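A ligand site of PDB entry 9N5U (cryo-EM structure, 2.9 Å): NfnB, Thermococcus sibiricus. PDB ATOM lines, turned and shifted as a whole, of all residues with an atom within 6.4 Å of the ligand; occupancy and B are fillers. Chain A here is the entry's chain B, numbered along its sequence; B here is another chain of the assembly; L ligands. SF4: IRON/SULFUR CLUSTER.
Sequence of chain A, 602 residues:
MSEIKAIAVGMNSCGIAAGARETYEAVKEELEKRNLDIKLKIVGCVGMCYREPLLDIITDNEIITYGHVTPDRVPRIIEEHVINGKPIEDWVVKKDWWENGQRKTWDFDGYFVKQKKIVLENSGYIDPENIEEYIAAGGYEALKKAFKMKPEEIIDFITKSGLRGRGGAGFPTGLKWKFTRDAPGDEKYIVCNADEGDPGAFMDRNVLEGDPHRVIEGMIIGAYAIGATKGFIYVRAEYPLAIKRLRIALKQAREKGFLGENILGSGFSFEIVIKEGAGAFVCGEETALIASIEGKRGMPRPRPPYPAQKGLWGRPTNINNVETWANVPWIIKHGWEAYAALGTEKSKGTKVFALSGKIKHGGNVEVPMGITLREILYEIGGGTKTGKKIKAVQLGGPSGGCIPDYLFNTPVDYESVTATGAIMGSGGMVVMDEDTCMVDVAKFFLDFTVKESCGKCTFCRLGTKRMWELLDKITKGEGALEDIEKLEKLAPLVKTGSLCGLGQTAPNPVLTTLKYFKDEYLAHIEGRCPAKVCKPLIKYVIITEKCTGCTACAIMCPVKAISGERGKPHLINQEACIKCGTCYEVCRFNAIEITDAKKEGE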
ATOM      1  N   VAL A 282      11.151  34.181   3.282  1.00  0.00           N
ATOM      2  CA  VAL A 282      11.232  33.954   4.715  1.00  0.00           C
ATOM      3  C   VAL A 282      10.415  34.984   5.496  1.00  0.00           C
ATOM      4  O   VAL A 282      10.024  34.717   6.631  1.00  0.00           O
ATOM      5  CB  VAL A 282      12.700  33.938   5.160  1.00  0.00           C
ATOM      6  CG1 VAL A 282      13.307  35.328   5.059  1.00  0.00           C
ATOM      7  CG2 VAL A 282      12.852  33.375   6.560  1.00  0.00           C
ATOM      8  N   GLY A 298      14.649  40.045   8.041  1.00  0.00           N
ATOM      9  CA  GLY A 298      13.649  39.011   8.223  1.00  0.00           C
ATOM     10  C   GLY A 298      14.220  37.706   8.722  1.00  0.00           C
ATOM     11  O   GLY A 298      14.190  36.707   7.997  1.00  0.00           O
ATOM     12  N   MET A 299      14.748  37.702   9.942  1.00  0.00           N
ATOM     13  CA  MET A 299      15.337  36.493  10.514  1.00  0.00           C
ATOM     14  C   MET A 299      14.435  35.951  11.603  1.00  0.00           C
ATOM     15  O   MET A 299      14.170  36.661  12.587  1.00  0.00           O
ATOM     16  CB  MET A 299      16.733  36.777  11.058  1.00  0.00           C
ATOM     17  CG  MET A 299      17.696  37.296  10.003  1.00  0.00           C
ATOM     18  SD  MET A 299      19.441  37.024  10.384  1.00  0.00           S
ATOM     19  CE  MET A 299      19.532  37.738  12.019  1.00  0.00           C
ATOM     20  N   PRO A 300      13.932  34.737  11.467  1.00  0.00           N
ATOM     21  CA  PRO A 300      13.022  34.177  12.476  1.00  0.00           C
ATOM     22  C   PRO A 300      13.711  33.942  13.809  1.00  0.00           C
ATOM     23  O   PRO A 300      14.936  33.831  13.905  1.00  0.00           O
ATOM     24  CB  PRO A 300      12.557  32.867  11.853  1.00  0.00           C
ATOM     25  CG  PRO A 300      12.756  33.055  10.393  1.00  0.00           C
ATOM     26  CD  PRO A 300      13.972  33.896  10.254  1.00  0.00           C
ATOM     27  N   ARG A 301      12.895  33.875  14.843  1.00  0.00           N
ATOM     28  CA  ARG A 301      13.345  33.640  16.214  1.00  0.00           C
ATOM     29  C   ARG A 301      12.584  32.468  16.797  1.00  0.00           C
ATOM     30  O   ARG A 301      11.533  32.071  16.283  1.00  0.00           O
ATOM     31  CB  ARG A 301      13.147  34.896  17.071  1.00  0.00           C
ATOM     32  CG  ARG A 301      11.731  35.385  17.126  1.00  0.00           C
ATOM     33  CD  ARG A 301      11.545  36.394  18.233  1.00  0.00           C
ATOM     34  NE  ARG A 301      10.226  37.007  18.174  1.00  0.00           N
ATOM     35  CZ  ARG A 301       9.133  36.478  18.689  1.00  0.00           C
ATOM     36  NH1 ARG A 301       9.155  35.312  19.309  1.00  0.00           N
ATOM     37  NH2 ARG A 301       7.972  37.120  18.568  1.00  0.00           N
ATOM     38  N   GLU A 452      16.403  31.395  -0.859  1.00  0.00           N
ATOM     39  CA  GLU A 452      15.503  32.123   0.016  1.00  0.00           C
ATOM     40  C   GLU A 452      15.798  31.960   1.504  1.00  0.00           C
ATOM     41  O   GLU A 452      15.145  32.614   2.317  1.00  0.00           O
ATOM     42  CB  GLU A 452      14.055  31.694  -0.252  1.00  0.00           C
ATOM     43  CG  GLU A 452      13.566  32.063  -1.628  1.00  0.00           C
ATOM     44  CD  GLU A 452      13.476  33.559  -1.839  1.00  0.00           C
ATOM     45  OE1 GLU A 452      13.280  34.295  -0.856  1.00  0.00           O
ATOM     46  OE2 GLU A 452      13.603  34.007  -3.005  1.00  0.00           O
ATOM     47  N   SER A 453      16.741  31.105   1.863  1.00  0.00           N
ATOM     48  CA  SER A 453      17.097  30.943   3.262  1.00  0.00           C
ATOM     49  C   SER A 453      17.686  32.231   3.818  1.00  0.00           C
ATOM     50  O   SER A 453      18.413  32.947   3.113  1.00  0.00           O
ATOM     51  CB  SER A 453      18.082  29.790   3.422  1.00  0.00           C
ATOM     52  OG  SER A 453      18.628  29.766   4.734  1.00  0.00           O
ATOM     53  N   CYS A 454      17.381  32.538   5.067  1.00  0.00           N
ATOM     54  CA  CYS A 454      17.923  33.735   5.688  1.00  0.00           C
ATOM     55  C   CYS A 454      19.356  33.559   6.168  1.00  0.00           C
ATOM     56  O   CYS A 454      20.012  34.551   6.508  1.00  0.00           O
ATOM     57  CB  CYS A 454      17.051  34.196   6.859  1.00  0.00           C
ATOM     58  SG  CYS A 454      17.126  33.162   8.324  1.00  0.00           S
ATOM     59  N   GLY A 455      19.868  32.328   6.183  1.00  0.00           N
ATOM     60  CA  GLY A 455      21.230  32.091   6.628  1.00  0.00           C
ATOM     61  C   GLY A 455      21.479  32.361   8.093  1.00  0.00           C
ATOM     62  O   GLY A 455      22.516  32.940   8.438  1.00  0.00           O
ATOM     63  N   LYS A 456      20.548  31.983   8.962  1.00  0.00           N
ATOM     64  CA  LYS A 456      20.723  32.141  10.401  1.00  0.00           C
ATOM     65  C   LYS A 456      21.143  30.855  11.084  1.00  0.00           C
ATOM     66  O   LYS A 456      22.180  30.823  11.760  1.00  0.00           O
ATOM     67  CB  LYS A 456      19.438  32.676  11.030  1.00  0.00           C
ATOM     68  CG  LYS A 456      19.523  32.862  12.529  1.00  0.00           C
ATOM     69  CD  LYS A 456      18.272  33.513  13.082  1.00  0.00           C
ATOM     70  CE  LYS A 456      18.317  33.593  14.591  1.00  0.00           C
ATOM     71  NZ  LYS A 456      17.160  34.346  15.124  1.00  0.00           N
ATOM     72  N   CYS A 457      20.385  29.776  10.921  1.00  0.00           N
ATOM     73  CA  CYS A 457      20.716  28.526  11.571  1.00  0.00           C
ATOM     74  C   CYS A 457      21.615  27.683  10.670  1.00  0.00           C
ATOM     75  O   CYS A 457      21.523  27.741   9.436  1.00  0.00           O
ATOM     76  CB  CYS A 457      19.463  27.748  11.960  1.00  0.00           C
ATOM     77  SG  CYS A 457      18.480  27.086  10.618  1.00  0.00           S
ATOM     78  N   THR A 458      22.499  26.911  11.302  1.00  0.00           N
ATOM     79  CA  THR A 458      23.503  26.155  10.550  1.00  0.00           C
ATOM     80  C   THR A 458      22.858  25.090   9.673  1.00  0.00           C
ATOM     81  O   THR A 458      23.304  24.863   8.551  1.00  0.00           O
ATOM     82  CB  THR A 458      24.510  25.522  11.507  1.00  0.00           C
ATOM     83  OG1 THR A 458      23.846  24.634  12.410  1.00  0.00           O
ATOM     84  CG2 THR A 458      25.226  26.593  12.305  1.00  0.00           C
ATOM     85  N   PHE A 459      21.802  24.443  10.178  1.00  0.00           N
ATOM     86  CA  PHE A 459      21.195  23.330   9.462  1.00  0.00           C
ATOM     87  C   PHE A 459      20.588  23.770   8.131  1.00  0.00           C
ATOM     88  O   PHE A 459      20.927  23.218   7.085  1.00  0.00           O
ATOM     89  CB  PHE A 459      20.137  22.648  10.329  1.00  0.00           C
ATOM     90  CG  PHE A 459      20.665  21.487  11.096  1.00  0.00           C
ATOM     91  CD1 PHE A 459      20.983  20.307  10.455  1.00  0.00           C
ATOM     92  CD2 PHE A 459      20.844  21.565  12.473  1.00  0.00           C
ATOM     93  CE1 PHE A 459      21.463  19.232  11.152  1.00  0.00           C
ATOM     94  CE2 PHE A 459      21.324  20.497  13.176  1.00  0.00           C
ATOM     95  CZ  PHE A 459      21.635  19.319  12.520  1.00  0.00           C
ATOM     96  N   CYS A 460      19.722  24.789   8.145  1.00  0.00           N
ATOM     97  CA  CYS A 460      19.120  25.227   6.888  1.00  0.00           C
ATOM     98  C   CYS A 460      20.190  25.768   5.949  1.00  0.00           C
ATOM     99  O   CYS A 460      20.379  25.239   4.842  1.00  0.00           O
ATOM    100  CB  CYS A 460      18.055  26.296   7.155  1.00  0.00           C
ATOM    101  SG  CYS A 460      17.277  26.992   5.688  1.00  0.00           S
ATOM    102  N   ARG A 461      20.995  26.721   6.436  1.00  0.00           N
ATOM    103  CA  ARG A 461      21.959  27.433   5.600  1.00  0.00           C
ATOM    104  C   ARG A 461      22.947  26.476   4.938  1.00  0.00           C
ATOM    105  O   ARG A 461      23.243  26.606   3.745  1.00  0.00           O
ATOM    106  CB  ARG A 461      22.706  28.459   6.442  1.00  0.00           C
ATOM    107  CG  ARG A 461      23.775  29.238   5.689  1.00  0.00           C
ATOM    108  CD  ARG A 461      24.510  30.223   6.588  1.00  0.00           C
ATOM    109  NE  ARG A 461      25.549  29.591   7.399  1.00  0.00           N
ATOM    110  CZ  ARG A 461      25.492  29.422   8.707  1.00  0.00           C
ATOM    111  NH1 ARG A 461      24.457  29.844   9.413  1.00  0.00           N
ATOM    112  NH2 ARG A 461      26.488  28.798   9.329  1.00  0.00           N
ATOM    113  N   SER A 498      16.371  22.295  11.800  1.00  0.00           N
ATOM    114  CA  SER A 498      16.209  23.687  11.411  1.00  0.00           C
ATOM    115  C   SER A 498      15.321  24.432  12.397  1.00  0.00           C
ATOM    116  O   SER A 498      14.482  23.853  13.096  1.00  0.00           O
ATOM    117  CB  SER A 498      15.643  23.799   9.999  1.00  0.00           C
ATOM    118  OG  SER A 498      16.535  23.234   9.059  1.00  0.00           O
ATOM    119  N   LEU A 499      15.510  25.754  12.450  1.00  0.00           N
ATOM    120  CA  LEU A 499      14.832  26.608  13.417  1.00  0.00           C
ATOM    121  C   LEU A 499      13.447  27.033  12.954  1.00  0.00           C
ATOM    122  O   LEU A 499      12.497  27.018  13.742  1.00  0.00           O
ATOM    123  CB  LEU A 499      15.680  27.830  13.718  1.00  0.00           C
ATOM    124  CG  LEU A 499      15.049  28.937  14.556  1.00  0.00           C
ATOM    125  CD1 LEU A 499      14.810  28.468  15.974  1.00  0.00           C
ATOM    126  CD2 LEU A 499      15.916  30.175  14.542  1.00  0.00           C
ATOM    127  N   CYS A 500      13.313  27.452  11.700  1.00  0.00           N
ATOM    128  CA  CYS A 500      12.039  27.946  11.191  1.00  0.00           C
ATOM    129  C   CYS A 500      11.462  26.961  10.188  1.00  0.00           C
ATOM    130  O   CYS A 500      12.077  25.958   9.841  1.00  0.00           O
ATOM    131  CB  CYS A 500      12.197  29.337  10.579  1.00  0.00           C
ATOM    132  SG  CYS A 500      12.286  29.383   8.783  1.00  0.00           S
ATOM    133  N   GLY A 501      10.244  27.265   9.741  1.00  0.00           N
ATOM    134  CA  GLY A 501       9.516  26.344   8.878  1.00  0.00           C
ATOM    135  C   GLY A 501      10.080  26.224   7.474  1.00  0.00           C
ATOM    136  O   GLY A 501       9.805  25.218   6.807  1.00  0.00           O
ATOM    137  N   LEU A 502      10.835  27.220   7.011  1.00  0.00           N
ATOM    138  CA  LEU A 502      11.439  27.118   5.686  1.00  0.00           C
ATOM    139  C   LEU A 502      12.418  25.956   5.614  1.00  0.00           C
ATOM    140  O   LEU A 502      12.399  25.177   4.653  1.00  0.00           O
ATOM    141  CB  LEU A 502      12.126  28.420   5.301  1.00  0.00           C
ATOM    142  CG  LEU A 502      13.044  28.473   4.065  1.00  0.00           C
ATOM    143  CD1 LEU A 502      12.413  27.847   2.844  1.00  0.00           C
ATOM    144  CD2 LEU A 502      13.432  29.898   3.751  1.00  0.00           C
ATOM    145  N   GLY A 503      13.272  25.811   6.624  1.00  0.00           N
ATOM    146  CA  GLY A 503      14.201  24.696   6.649  1.00  0.00           C
ATOM    147  C   GLY A 503      13.575  23.400   7.097  1.00  0.00           C
ATOM    148  O   GLY A 503      14.042  22.324   6.715  1.00  0.00           O
ATOM    149  N   GLN A 504      12.532  23.465   7.921  1.00  0.00           N
ATOM    150  CA  GLN A 504      11.846  22.263   8.361  1.00  0.00           C
ATOM    151  C   GLN A 504      10.959  21.660   7.282  1.00  0.00           C
ATOM    152  O   GLN A 504      10.633  20.480   7.347  1.00  0.00           O
ATOM    153  CB  GLN A 504      11.012  22.560   9.610  1.00  0.00           C
ATOM    154  CG  GLN A 504      11.839  22.913  10.830  1.00  0.00           C
ATOM    155  CD  GLN A 504      11.002  23.278  12.026  1.00  0.00           C
ATOM    156  OE1 GLN A 504       9.772  23.229  11.963  1.00  0.00           O
ATOM    157  NE2 GLN A 504      11.648  23.640  13.114  1.00  0.00           N
ATOM    158  N   GLY B  50      18.814  30.935  18.115  1.00  0.00           N
ATOM    159  CA  GLY B  50      18.795  29.580  17.621  1.00  0.00           C
ATOM    160  C   GLY B  50      19.617  29.322  16.375  1.00  0.00           C
ATOM    161  O   GLY B  50      19.153  28.650  15.450  1.00  0.00           O
ATOM    162  N   ARG B  53      22.435  25.576  16.525  1.00  0.00           N
ATOM    163  CA  ARG B  53      21.665  24.323  16.465  1.00  0.00           C
ATOM    164  C   ARG B  53      22.468  23.136  16.994  1.00  0.00           C
ATOM    165  O   ARG B  53      22.410  22.039  16.439  1.00  0.00           O
ATOM    166  CB  ARG B  53      21.173  24.046  15.045  1.00  0.00           C
ATOM    167  CG  ARG B  53      20.514  25.222  14.366  1.00  0.00           C
ATOM    168  CD  ARG B  53      19.019  25.219  14.566  1.00  0.00           C
ATOM    169  NE  ARG B  53      18.581  25.923  15.760  1.00  0.00           N
ATOM    170  CZ  ARG B  53      17.419  25.701  16.367  1.00  0.00           C
ATOM    171  NH1 ARG B  53      16.591  24.767  15.961  1.00  0.00           N
ATOM    172  NH2 ARG B  53      17.080  26.457  17.407  1.00  0.00           N
HETATM  173 FE1  SF4 L   1      14.550  29.384   8.872  1.00  0.00          FE
HETATM  174 FE2  SF4 L   1      16.498  28.568   7.124  1.00  0.00          FE
HETATM  175 FE3  SF4 L   1      16.988  28.570   9.816  1.00  0.00          FE
HETATM  176 FE4  SF4 L   1      16.766  30.940   8.473  1.00  0.00          FE
HETATM  177  S1  SF4 L   1      18.361  29.349   8.173  1.00  0.00           S
HETATM  178  S2  SF4 L   1      15.818  30.408  10.478  1.00  0.00           S
HETATM  179  S3  SF4 L   1      15.167  30.417   6.928  1.00  0.00           S
HETATM  180  S4  SF4 L   1      15.449  27.304   8.705  1.00  0.00           S
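The backbone NH (N) of Cys 457 sits close to a sulfur (S1) of the ligand (3.4 Å). An iron atom (FE3) of the ligand is bound by the side-chain sulfur of Cys 457 (2.3 Å). N of Cys 454 sits close to S3 of the ligand. An iron atom (FE4) of the ligand is bound by the side-chain sulfur of Cys 454, at 2.3 Å. N of Cys 500 sits close to S4 of the ligand (3.7 Å). The side-chain sulfur (SG) of Cys 500 binds an iron atom (FE1) of the ligand. An iron atom (FE2) of the ligand is bound by the side-chain sulfur of Cys 460. S4 of the ligand lies close to N of Gly 503. A sulfur (S1) of the ligand lies close to the side-chain hydroxyl of Ser 453. A sulfur (S1) of the ligand sits close to the backbone NH of Lys 456 (3.5 Å).
Residues that only touch the ligand: Val 282 (3.8 Å), Pro 300 (3.95 Å), Gly 455 (3.9 Å), Ser 498 (3.7 Å) and Leu 502 (3.7 Å). The nearest printed residue that does not touch the ligand is Leu 499 (4.1 Å).
SG of Cys 457 sits close to N of Cys 460 (3.6 Å). The backbone NH of Leu 499 lies close to the side-chain sulfur of Cys 457 (3.7 Å). SG of Cys 454 lies close to N of Lys 456. N of Leu 502 lies close to SG of Cys 500 (3.2 Å). The side-chain hydroxyl of Ser 453 sits at hydrogen-bond distance from the backbone NH of Gly 455. The backbone carbonyl oxygen (O) of Pro 300 lies within hydrogen-bond range of the side-chain amino group (NZ) of Lys 456 (2.6 Å). The backbone carbonyl oxygen (O) of Lys 456 sits at hydrogen-bond distance from the guanidinium group (NH1) of Arg 461 (3.4 Å). The side-chain amide nitrogen of Gln 504 lies within hydrogen-bond range of the backbone carbonyl oxygen of Ser 498.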
